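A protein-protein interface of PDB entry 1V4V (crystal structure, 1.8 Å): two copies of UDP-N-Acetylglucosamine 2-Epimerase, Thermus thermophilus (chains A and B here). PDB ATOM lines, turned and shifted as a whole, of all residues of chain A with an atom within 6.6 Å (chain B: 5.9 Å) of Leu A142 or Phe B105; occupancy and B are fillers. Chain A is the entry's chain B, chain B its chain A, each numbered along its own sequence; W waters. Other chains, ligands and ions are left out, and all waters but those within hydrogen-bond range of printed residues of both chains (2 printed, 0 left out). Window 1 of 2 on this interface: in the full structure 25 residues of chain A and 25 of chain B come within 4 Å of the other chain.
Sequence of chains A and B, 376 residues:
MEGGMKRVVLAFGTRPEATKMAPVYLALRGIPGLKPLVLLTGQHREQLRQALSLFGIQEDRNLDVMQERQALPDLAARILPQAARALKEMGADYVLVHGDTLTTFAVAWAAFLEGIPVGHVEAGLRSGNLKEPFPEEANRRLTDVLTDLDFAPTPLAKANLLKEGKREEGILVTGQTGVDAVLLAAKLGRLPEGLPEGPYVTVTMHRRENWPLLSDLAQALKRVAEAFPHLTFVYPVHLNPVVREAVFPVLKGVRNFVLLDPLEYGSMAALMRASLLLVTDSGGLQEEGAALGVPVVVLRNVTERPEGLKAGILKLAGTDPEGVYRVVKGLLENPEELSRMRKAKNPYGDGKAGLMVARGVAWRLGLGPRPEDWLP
The backbone NH (N) of Leu B102 lies close to the side-chain amide nitrogen (ND2) of Asn B139 (3.1 Å).
Among the printed residues, merely in contact across the chains: Trp A109 with Leu B102, Leu A142 with Leu B142, Phe A105 with Trp B109, Trp A109 with Phe B105, Val A145 with Arg B141, Arg A141 with Val B145, Val A145 with Val B145, Val A145 with Leu B142, Leu A142 with Val B145, Trp A109 with Leu B142, Ala A138 with Leu B146, Phe A105 with Leu B142, Leu A142 with Trp B109 and Leu A142 with Phe B105.
Glu A137 touches none of the printed residues of chain B.
Of the printed residues of chain B, Ala A138 touches Leu B146 (3.9 Å).
Of the printed residues of chain B, Leu A142 touches Phe B105, Trp B109, Leu B142 and Val B145.
Thr A143 touches none of the printed residues of chain B.
Of the printed residues of chain B, Val A145 touches Arg B141 (3.6 Å), Leu B142 (3.8 Å) and Val B145 (3.6 Å).
Of the printed residues of chain A, Phe B105 touches Trp A109 and Leu A142.
Printed residues of chain A within 4 Å of Trp B109: Phe A105 and Leu A142.
Of the printed residues of chain A, Leu B142 touches Phe A105 (3.9 Å), Trp A109 (3.8 Å), Leu A142 (3.4 Å) and Val A145 (3.8 Å).
Printed residues of chain A within 4 Å of Leu B146: Ala A138 (3.9 Å).
The nearest printed residue of chain B that does not touch Trp A109 is Trp B109 (4.1 Å).
Of the 16 printed residues of chain A, 6 touch a printed residue of chain B.
Printed residues of chain A that touch a printed residue of chain B: Phe A105, Trp A109, Ala A138, Arg A141, Leu A142 and Val A145.
Hydrophobic or aromatic side chains of chain A within 4 Å of the printed part of chain B: Phe A105, Trp A109, Ala A138, Leu A142 and Val A145.
Along chain A the printed residues that touch a printed residue of chain B span positions 105 to 145.
Of the 16 printed residues of chain B, 7 touch a printed residue of chain A.
Printed residues of chain B that touch a printed residue of chain A: Leu B102, Phe B105, Trp B109, Arg B141, Leu B142, Val B145 and Leu B146.
Among the printed residues, no Asp or Glu carboxylate lies within 4 Å of a Lys or Arg side-chain nitrogen of the other chain.
Phe A105 touches Trp B109, and with the chains exchanged Trp A109 touches Phe B105.
Trp A109 touches Leu B142, and with the chains exchanged Leu A142 touches Trp B109.
Arg A141 touches Val B145, and with the chains exchanged Val A145 touches Arg B141.
Val A145 touches its own counterpart, Val B145.
Positions printed for both chains: 105, 108, 109, 139, 141, 142, 143, 145 and 146.
Water W2 lies within hydrogen-bond range of the side-chain amide oxygen of Asn A139 (2.6 Å) and the indole nitrogen of Trp B109 (3.0 Å).
Water W1 lies within hydrogen-bond range of the side-chain amide oxygen (OD1) of Asn B139 (2.7 Å) and the indole nitrogen (NE1) of Trp A109 (2.9 Å).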
ATOM      1  N   PHE A 105     -26.156  25.119  11.302  1.00  0.00           N
ATOM      2  CA  PHE A 105     -26.154  24.358  12.545  1.00  0.00           C
ATOM      3  C   PHE A 105     -26.473  25.271  13.721  1.00  0.00           C
ATOM      4  O   PHE A 105     -27.223  24.899  14.628  1.00  0.00           O
ATOM      5  CB  PHE A 105     -24.807  23.682  12.810  1.00  0.00           C
ATOM      6  CG  PHE A 105     -24.691  23.146  14.215  1.00  0.00           C
ATOM      7  CD1 PHE A 105     -25.547  22.139  14.657  1.00  0.00           C
ATOM      8  CD2 PHE A 105     -23.791  23.708  15.122  1.00  0.00           C
ATOM      9  CE1 PHE A 105     -25.518  21.701  15.985  1.00  0.00           C
ATOM     10  CE2 PHE A 105     -23.750  23.278  16.456  1.00  0.00           C
ATOM     11  CZ  PHE A 105     -24.613  22.275  16.890  1.00  0.00           C
ATOM     12  N   ALA A 108     -30.116  25.748  13.942  1.00  0.00           N
ATOM     13  CA  ALA A 108     -30.770  24.516  14.378  1.00  0.00           C
ATOM     14  C   ALA A 108     -30.567  24.309  15.883  1.00  0.00           C
ATOM     15  O   ALA A 108     -31.474  23.876  16.597  1.00  0.00           O
ATOM     16  CB  ALA A 108     -30.205  23.318  13.615  1.00  0.00           C
ATOM     17  N   TRP A 109     -29.369  24.623  16.359  1.00  0.00           N
ATOM     18  CA  TRP A 109     -29.077  24.455  17.773  1.00  0.00           C
ATOM     19  C   TRP A 109     -29.867  25.474  18.594  1.00  0.00           C
ATOM     20  O   TRP A 109     -30.382  25.149  19.665  1.00  0.00           O
ATOM     21  CB  TRP A 109     -27.573  24.589  18.008  1.00  0.00           C
ATOM     22  CG  TRP A 109     -27.132  24.112  19.357  1.00  0.00           C
ATOM     23  CD1 TRP A 109     -27.750  23.180  20.154  1.00  0.00           C
ATOM     24  CD2 TRP A 109     -25.945  24.505  20.047  1.00  0.00           C
ATOM     25  NE1 TRP A 109     -27.011  22.974  21.301  1.00  0.00           N
ATOM     26  CE2 TRP A 109     -25.900  23.776  21.256  1.00  0.00           C
ATOM     27  CE3 TRP A 109     -24.912  25.406  19.758  1.00  0.00           C
ATOM     28  CZ2 TRP A 109     -24.857  23.924  22.179  1.00  0.00           C
ATOM     29  CZ3 TRP A 109     -23.874  25.551  20.681  1.00  0.00           C
ATOM     30  CH2 TRP A 109     -23.859  24.813  21.873  1.00  0.00           C
ATOM     31  N   ARG A 126     -23.248  12.374   3.240  1.00  0.00           N
ATOM     32  CA  ARG A 126     -22.055  12.198   4.061  1.00  0.00           C
ATOM     33  C   ARG A 126     -20.813  11.897   3.236  1.00  0.00           C
ATOM     34  O   ARG A 126     -20.892  11.297   2.164  1.00  0.00           O
ATOM     35  CB  ARG A 126     -22.264  11.053   5.056  1.00  0.00           C
ATOM     36  CG  ARG A 126     -23.392  11.269   6.049  1.00  0.00           C
ATOM     37  CD  ARG A 126     -23.020  12.311   7.085  1.00  0.00           C
ATOM     38  NE  ARG A 126     -24.071  12.471   8.085  1.00  0.00           N
ATOM     39  CZ  ARG A 126     -25.097  13.307   7.977  1.00  0.00           C
ATOM     40  NH1 ARG A 126     -25.223  14.075   6.904  1.00  0.00           N
ATOM     41  NH2 ARG A 126     -25.999  13.372   8.947  1.00  0.00           N
ATOM     42  N   PRO A 135     -15.733  22.892   7.460  1.00  0.00           N
ATOM     43  CA  PRO A 135     -16.388  22.162   8.551  1.00  0.00           C
ATOM     44  C   PRO A 135     -17.781  21.649   8.181  1.00  0.00           C
ATOM     45  O   PRO A 135     -18.570  21.309   9.065  1.00  0.00           O
ATOM     46  CB  PRO A 135     -16.461  23.213   9.641  1.00  0.00           C
ATOM     47  CG  PRO A 135     -16.866  24.417   8.847  1.00  0.00           C
ATOM     48  CD  PRO A 135     -15.970  24.341   7.604  1.00  0.00           C
ATOM     49  N   GLU A 137     -18.954  18.765   6.759  1.00  0.00           N
ATOM     50  CA  GLU A 137     -19.328  17.404   7.151  1.00  0.00           C
ATOM     51  C   GLU A 137     -19.775  17.397   8.614  1.00  0.00           C
ATOM     52  O   GLU A 137     -20.785  16.783   8.957  1.00  0.00           O
ATOM     53  CB  GLU A 137     -18.152  16.440   6.957  1.00  0.00           C
ATOM     54  CG  GLU A 137     -18.399  15.003   7.421  1.00  0.00           C
ATOM     55  CD  GLU A 137     -19.334  14.215   6.517  1.00  0.00           C
ATOM     56  OE1 GLU A 137     -19.514  13.004   6.770  1.00  0.00           O
ATOM     57  OE2 GLU A 137     -19.881  14.789   5.556  1.00  0.00           O
ATOM     58  N   ALA A 138     -19.024  18.080   9.473  1.00  0.00           N
ATOM     59  CA  ALA A 138     -19.387  18.148  10.886  1.00  0.00           C
ATOM     60  C   ALA A 138     -20.700  18.912  11.051  1.00  0.00           C
ATOM     61  O   ALA A 138     -21.576  18.490  11.805  1.00  0.00           O
ATOM     62  CB  ALA A 138     -18.279  18.833  11.690  1.00  0.00           C
ATOM     63  N   ASN A 139     -20.840  20.031  10.339  1.00  0.00           N
ATOM     64  CA  ASN A 139     -22.051  20.845  10.432  1.00  0.00           C
ATOM     65  C   ASN A 139     -23.312  20.036  10.156  1.00  0.00           C
ATOM     66  O   ASN A 139     -24.285  20.118  10.905  1.00  0.00           O
ATOM     67  CB  ASN A 139     -22.018  22.027   9.450  1.00  0.00           C
ATOM     68  CG  ASN A 139     -20.930  23.039   9.768  1.00  0.00           C
ATOM     69  OD1 ASN A 139     -20.482  23.157  10.910  1.00  0.00           O
ATOM     70  ND2 ASN A 139     -20.514  23.791   8.754  1.00  0.00           N
ATOM     71  N   ARG A 140     -23.309  19.255   9.082  1.00  0.00           N
ATOM     72  CA  ARG A 140     -24.513  18.490   8.777  1.00  0.00           C
ATOM     73  C   ARG A 140     -24.758  17.361   9.762  1.00  0.00           C
ATOM     74  O   ARG A 140     -25.906  17.073  10.089  1.00  0.00           O
ATOM     75  CB  ARG A 140     -24.493  17.972   7.334  1.00  0.00           C
ATOM     76  CG  ARG A 140     -23.257  17.221   6.915  1.00  0.00           C
ATOM     77  CD  ARG A 140     -23.226  17.131   5.387  1.00  0.00           C
ATOM     78  NE  ARG A 140     -22.027  16.471   4.888  1.00  0.00           N
ATOM     79  CZ  ARG A 140     -21.566  16.614   3.648  1.00  0.00           C
ATOM     80  NH1 ARG A 140     -20.465  15.980   3.266  1.00  0.00           N
ATOM     81  NH2 ARG A 140     -22.204  17.402   2.791  1.00  0.00           N
ATOM     82  N   ARG A 141     -23.694  16.734  10.255  1.00  0.00           N
ATOM     83  CA  ARG A 141     -23.868  15.660  11.221  1.00  0.00           C
ATOM     84  C   ARG A 141     -24.416  16.216  12.529  1.00  0.00           C
ATOM     85  O   ARG A 141     -25.318  15.625  13.120  1.00  0.00           O
ATOM     86  CB  ARG A 141     -22.541  14.921  11.471  1.00  0.00           C
ATOM     87  CG  ARG A 141     -22.106  14.019  10.310  1.00  0.00           C
ATOM     88  CD  ARG A 141     -20.831  13.251  10.647  1.00  0.00           C
ATOM     89  NE  ARG A 141     -21.022  12.354  11.785  1.00  0.00           N
ATOM     90  CZ  ARG A 141     -20.032  11.761  12.450  1.00  0.00           C
ATOM     91  NH1 ARG A 141     -18.769  11.966  12.095  1.00  0.00           N
ATOM     92  NH2 ARG A 141     -20.304  10.969  13.479  1.00  0.00           N
ATOM     93  N   LEU A 142     -23.873  17.352  12.974  1.00  0.00           N
ATOM     94  CA  LEU A 142     -24.324  17.986  14.216  1.00  0.00           C
ATOM     95  C   LEU A 142     -25.789  18.386  14.082  1.00  0.00           C
ATOM     96  O   LEU A 142     -26.598  18.166  14.987  1.00  0.00           O
ATOM     97  CB  LEU A 142     -23.492  19.236  14.511  1.00  0.00           C
ATOM     98  CG  LEU A 142     -22.024  19.049  14.906  1.00  0.00           C
ATOM     99  CD1 LEU A 142     -21.332  20.410  14.900  1.00  0.00           C
ATOM    100  CD2 LEU A 142     -21.934  18.402  16.297  1.00  0.00           C
ATOM    101  N   THR A 143     -26.127  18.987  12.948  1.00  0.00           N
ATOM    102  CA  THR A 143     -27.499  19.403  12.716  1.00  0.00           C
ATOM    103  C   THR A 143     -28.455  18.214  12.800  1.00  0.00           C
ATOM    104  O   THR A 143     -29.523  18.306  13.407  1.00  0.00           O
ATOM    105  CB  THR A 143     -27.653  20.066  11.338  1.00  0.00           C
ATOM    106  OG1 THR A 143     -26.848  21.252  11.280  1.00  0.00           O
ATOM    107  CG2 THR A 143     -29.118  20.424  11.085  1.00  0.00           C
ATOM    108  N   ASP A 144     -28.076  17.091  12.201  1.00  0.00           N
ATOM    109  CA  ASP A 144     -28.958  15.930  12.222  1.00  0.00           C
ATOM    110  C   ASP A 144     -29.157  15.279  13.588  1.00  0.00           C
ATOM    111  O   ASP A 144     -30.131  14.556  13.797  1.00  0.00           O
ATOM    112  CB  ASP A 144     -28.509  14.904  11.171  1.00  0.00           C
ATOM    113  CG  ASP A 144     -28.736  15.411   9.754  1.00  0.00           C
ATOM    114  OD1 ASP A 144     -29.643  16.250   9.585  1.00  0.00           O
ATOM    115  OD2 ASP A 144     -28.031  14.982   8.818  1.00  0.00           O
ATOM    116  N   VAL A 145     -28.251  15.530  14.525  1.00  0.00           N
ATOM    117  CA  VAL A 145     -28.426  14.991  15.871  1.00  0.00           C
ATOM    118  C   VAL A 145     -29.706  15.612  16.454  1.00  0.00           C
ATOM    119  O   VAL A 145     -30.488  14.946  17.134  1.00  0.00           O
ATOM    120  CB  VAL A 145     -27.245  15.389  16.811  1.00  0.00           C
ATOM    121  CG1 VAL A 145     -27.593  15.080  18.270  1.00  0.00           C
ATOM    122  CG2 VAL A 145     -25.981  14.645  16.419  1.00  0.00           C
ATOM    123  N   LEU A 146     -29.912  16.893  16.158  1.00  0.00           N
ATOM    124  CA  LEU A 146     -31.028  17.668  16.693  1.00  0.00           C
ATOM    125  C   LEU A 146     -32.319  17.693  15.883  1.00  0.00           C
ATOM    126  O   LEU A 146     -33.317  18.237  16.332  1.00  0.00           O
ATOM    127  CB  LEU A 146     -30.576  19.121  16.876  1.00  0.00           C
ATOM    128  CG  LEU A 146     -29.224  19.359  17.557  1.00  0.00           C
ATOM    129  CD1 LEU A 146     -28.905  20.853  17.548  1.00  0.00           C
ATOM    130  CD2 LEU A 146     -29.269  18.821  18.986  1.00  0.00           C
ATOM    131  N   THR A 147     -32.307  17.104  14.700  1.00  0.00           N
ATOM    132  CA  THR A 147     -33.477  17.174  13.839  1.00  0.00           C
ATOM    133  C   THR A 147     -34.673  16.297  14.187  1.00  0.00           C
ATOM    134  O   THR A 147     -34.532  15.117  14.515  1.00  0.00           O
ATOM    135  CB  THR A 147     -33.055  16.905  12.397  1.00  0.00           C
ATOM    136  OG1 THR A 147     -32.071  17.871  12.006  1.00  0.00           O
ATOM    137  CG2 THR A 147     -34.242  17.005  11.460  1.00  0.00           C
ATOM    138  N   THR B 101     -22.271  18.507  29.795  1.00  0.00           N
ATOM    139  CA  THR B 101     -22.758  19.878  29.922  1.00  0.00           C
ATOM    140  C   THR B 101     -22.657  20.658  28.614  1.00  0.00           C
ATOM    141  O   THR B 101     -21.944  20.263  27.694  1.00  0.00           O
ATOM    142  CB  THR B 101     -21.983  20.676  30.992  1.00  0.00           C
ATOM    143  OG1 THR B 101     -20.619  20.819  30.579  1.00  0.00           O
ATOM    144  CG2 THR B 101     -22.037  19.973  32.344  1.00  0.00           C
ATOM    145  N   LEU B 102     -23.375  21.776  28.555  1.00  0.00           N
ATOM    146  CA  LEU B 102     -23.360  22.647  27.385  1.00  0.00           C
ATOM    147  C   LEU B 102     -21.933  23.178  27.181  1.00  0.00           C
ATOM    148  O   LEU B 102     -21.441  23.264  26.054  1.00  0.00           O
ATOM    149  CB  LEU B 102     -24.328  23.815  27.604  1.00  0.00           C
ATOM    150  CG  LEU B 102     -24.615  24.754  26.427  1.00  0.00           C
ATOM    151  CD1 LEU B 102     -25.396  24.011  25.369  1.00  0.00           C
ATOM    152  CD2 LEU B 102     -25.417  25.952  26.909  1.00  0.00           C
ATOM    153  N   THR B 103     -21.270  23.527  28.280  1.00  0.00           N
ATOM    154  CA  THR B 103     -19.908  24.049  28.200  1.00  0.00           C
ATOM    155  C   THR B 103     -18.971  23.010  27.599  1.00  0.00           C
ATOM    156  O   THR B 103     -18.101  23.345  26.797  1.00  0.00           O
ATOM    157  CB  THR B 103     -19.394  24.474  29.589  1.00  0.00           C
ATOM    158  OG1 THR B 103     -20.234  25.515  30.099  1.00  0.00           O
ATOM    159  CG2 THR B 103     -17.954  24.990  29.502  1.00  0.00           C
ATOM    160  N   THR B 104     -19.148  21.749  27.976  1.00  0.00           N
ATOM    161  CA  THR B 104     -18.307  20.692  27.442  1.00  0.00           C
ATOM    162  C   THR B 104     -18.435  20.601  25.932  1.00  0.00           C
ATOM    163  O   THR B 104     -17.431  20.462  25.230  1.00  0.00           O
ATOM    164  CB  THR B 104     -18.644  19.332  28.091  1.00  0.00           C
ATOM    165  OG1 THR B 104     -18.095  19.300  29.414  1.00  0.00           O
ATOM    166  CG2 THR B 104     -18.072  18.177  27.281  1.00  0.00           C
ATOM    167  N   PHE B 105     -19.658  20.683  25.413  1.00  0.00           N
ATOM    168  CA  PHE B 105     -19.808  20.624  23.965  1.00  0.00           C
ATOM    169  C   PHE B 105     -19.221  21.875  23.317  1.00  0.00           C
ATOM    170  O   PHE B 105     -18.560  21.793  22.281  1.00  0.00           O
ATOM    171  CB  PHE B 105     -21.275  20.509  23.532  1.00  0.00           C
ATOM    172  CG  PHE B 105     -21.461  20.704  22.055  1.00  0.00           C
ATOM    173  CD1 PHE B 105     -20.858  19.834  21.150  1.00  0.00           C
ATOM    174  CD2 PHE B 105     -22.140  21.816  21.564  1.00  0.00           C
ATOM    175  CE1 PHE B 105     -20.919  20.073  19.772  1.00  0.00           C
ATOM    176  CE2 PHE B 105     -22.208  22.063  20.189  1.00  0.00           C
ATOM    177  CZ  PHE B 105     -21.594  21.190  19.292  1.00  0.00           C
ATOM    178  N   ALA B 106     -19.471  23.031  23.921  1.00  0.00           N
ATOM    179  CA  ALA B 106     -18.968  24.285  23.369  1.00  0.00           C
ATOM    180  C   ALA B 106     -17.449  24.234  23.250  1.00  0.00           C
ATOM    181  O   ALA B 106     -16.882  24.715  22.269  1.00  0.00           O
ATOM    182  CB  ALA B 106     -19.396  25.459  24.243  1.00  0.00           C
ATOM    183  N   VAL B 107     -16.791  23.639  24.244  1.00  0.00           N
ATOM    184  CA  VAL B 107     -15.334  23.522  24.223  1.00  0.00           C
ATOM    185  C   VAL B 107     -14.892  22.544  23.140  1.00  0.00           C
ATOM    186  O   VAL B 107     -13.943  22.813  22.403  1.00  0.00           O
ATOM    187  CB  VAL B 107     -14.789  23.065  25.605  1.00  0.00           C
ATOM    188  CG1 VAL B 107     -13.296  22.796  25.519  1.00  0.00           C
ATOM    189  CG2 VAL B 107     -15.063  24.142  26.646  1.00  0.00           C
ATOM    190  N   ALA B 108     -15.587  21.412  23.034  1.00  0.00           N
ATOM    191  CA  ALA B 108     -15.268  20.414  22.022  1.00  0.00           C
ATOM    192  C   ALA B 108     -15.458  20.996  20.619  1.00  0.00           C
ATOM    193  O   ALA B 108     -14.670  20.717  19.707  1.00  0.00           O
ATOM    194  CB  ALA B 108     -16.153  19.183  22.195  1.00  0.00           C
ATOM    195  N   TRP B 109     -16.498  21.805  20.443  1.00  0.00           N
ATOM    196  CA  TRP B 109     -16.744  22.399  19.131  1.00  0.00           C
ATOM    197  C   TRP B 109     -15.659  23.438  18.820  1.00  0.00           C
ATOM    198  O   TRP B 109     -15.206  23.555  17.680  1.00  0.00           O
ATOM    199  CB  TRP B 109     -18.140  23.031  19.090  1.00  0.00           C
ATOM    200  CG  TRP B 109     -18.606  23.409  17.703  1.00  0.00           C
ATOM    201  CD1 TRP B 109     -18.180  22.882  16.516  1.00  0.00           C
ATOM    202  CD2 TRP B 109     -19.609  24.376  17.372  1.00  0.00           C
ATOM    203  NE1 TRP B 109     -18.855  23.461  15.467  1.00  0.00           N
ATOM    204  CE2 TRP B 109     -19.738  24.381  15.965  1.00  0.00           C
ATOM    205  CE3 TRP B 109     -20.413  25.237  18.128  1.00  0.00           C
ATOM    206  CZ2 TRP B 109     -20.640  25.217  15.297  1.00  0.00           C
ATOM    207  CZ3 TRP B 109     -21.311  26.069  17.463  1.00  0.00           C
ATOM    208  CH2 TRP B 109     -21.415  26.050  16.063  1.00  0.00           C
ATOM    209  N   ALA B 110     -15.238  24.178  19.842  1.00  0.00           N
ATOM    210  CA  ALA B 110     -14.193  25.184  19.678  1.00  0.00           C
ATOM    211  C   ALA B 110     -12.912  24.488  19.224  1.00  0.00           C
ATOM    212  O   ALA B 110     -12.232  24.954  18.311  1.00  0.00           O
ATOM    213  CB  ALA B 110     -13.956  25.912  20.995  1.00  0.00           C
ATOM    214  N   ASN B 139     -26.314  17.282  24.215  1.00  0.00           N
ATOM    215  CA  ASN B 139     -24.926  17.702  24.397  1.00  0.00           C
ATOM    216  C   ASN B 139     -23.925  16.583  24.141  1.00  0.00           C
ATOM    217  O   ASN B 139     -22.934  16.776  23.417  1.00  0.00           O
ATOM    218  CB  ASN B 139     -24.685  18.244  25.814  1.00  0.00           C
ATOM    219  CG  ASN B 139     -25.354  19.583  26.062  1.00  0.00           C
ATOM    220  OD1 ASN B 139     -25.699  20.308  25.130  1.00  0.00           O
ATOM    221  ND2 ASN B 139     -25.522  19.928  27.338  1.00  0.00           N
ATOM    222  N   ARG B 141     -24.382  13.701  22.494  1.00  0.00           N
ATOM    223  CA  ARG B 141     -24.433  13.194  21.130  1.00  0.00           C
ATOM    224  C   ARG B 141     -23.697  14.161  20.197  1.00  0.00           C
ATOM    225  O   ARG B 141     -22.960  13.732  19.310  1.00  0.00           O
ATOM    226  CB  ARG B 141     -25.883  13.011  20.683  1.00  0.00           C
ATOM    227  CG  ARG B 141     -26.557  11.818  21.348  1.00  0.00           C
ATOM    228  CD  ARG B 141     -28.006  11.688  20.912  1.00  0.00           C
ATOM    229  NE  ARG B 141     -28.121  11.585  19.462  1.00  0.00           N
ATOM    230  CZ  ARG B 141     -29.275  11.494  18.812  1.00  0.00           C
ATOM    231  NH1 ARG B 141     -30.420  11.486  19.487  1.00  0.00           N
ATOM    232  NH2 ARG B 141     -29.284  11.433  17.486  1.00  0.00           N
ATOM    233  N   LEU B 142     -23.892  15.462  20.413  1.00  0.00           N
ATOM    234  CA  LEU B 142     -23.223  16.481  19.599  1.00  0.00           C
ATOM    235  C   LEU B 142     -21.709  16.374  19.803  1.00  0.00           C
ATOM    236  O   LEU B 142     -20.943  16.363  18.843  1.00  0.00           O
ATOM    237  CB  LEU B 142     -23.697  17.882  19.998  1.00  0.00           C
ATOM    238  CG  LEU B 142     -25.136  18.264  19.628  1.00  0.00           C
ATOM    239  CD1 LEU B 142     -25.500  19.581  20.305  1.00  0.00           C
ATOM    240  CD2 LEU B 142     -25.271  18.388  18.095  1.00  0.00           C
ATOM    241  N   THR B 143     -21.285  16.292  21.062  1.00  0.00           N
ATOM    242  CA  THR B 143     -19.866  16.174  21.365  1.00  0.00           C
ATOM    243  C   THR B 143     -19.239  14.959  20.686  1.00  0.00           C
ATOM    244  O   THR B 143     -18.135  15.048  20.134  1.00  0.00           O
ATOM    245  CB  THR B 143     -19.624  16.070  22.882  1.00  0.00           C
ATOM    246  OG1 THR B 143     -20.114  17.255  23.523  1.00  0.00           O
ATOM    247  CG2 THR B 143     -18.125  15.927  23.182  1.00  0.00           C
ATOM    248  N   VAL B 145     -20.092  13.529  17.946  1.00  0.00           N
ATOM    249  CA  VAL B 145     -20.009  13.645  16.494  1.00  0.00           C
ATOM    250  C   VAL B 145     -18.589  14.132  16.176  1.00  0.00           C
ATOM    251  O   VAL B 145     -17.963  13.684  15.218  1.00  0.00           O
ATOM    252  CB  VAL B 145     -21.008  14.695  15.952  1.00  0.00           C
ATOM    253  CG1 VAL B 145     -20.606  15.127  14.543  1.00  0.00           C
ATOM    254  CG2 VAL B 145     -22.409  14.122  15.945  1.00  0.00           C
ATOM    255  N   LEU B 146     -18.090  15.037  17.013  1.00  0.00           N
ATOM    256  CA  LEU B 146     -16.776  15.654  16.831  1.00  0.00           C
ATOM    257  C   LEU B 146     -15.565  14.934  17.415  1.00  0.00           C
ATOM    258  O   LEU B 146     -14.430  15.308  17.129  1.00  0.00           O
ATOM    259  CB  LEU B 146     -16.794  17.063  17.423  1.00  0.00           C
ATOM    260  CG  LEU B 146     -17.963  17.960  17.033  1.00  0.00           C
ATOM    261  CD1 LEU B 146     -17.807  19.294  17.737  1.00  0.00           C
ATOM    262  CD2 LEU B 146     -18.004  18.132  15.513  1.00  0.00           C
HETATM  263  O   HOH W   1     -27.559  20.890  23.278  1.00  0.00           O
HETATM  264  O   HOH W   2     -18.668  22.418  12.615  1.00  0.00           O
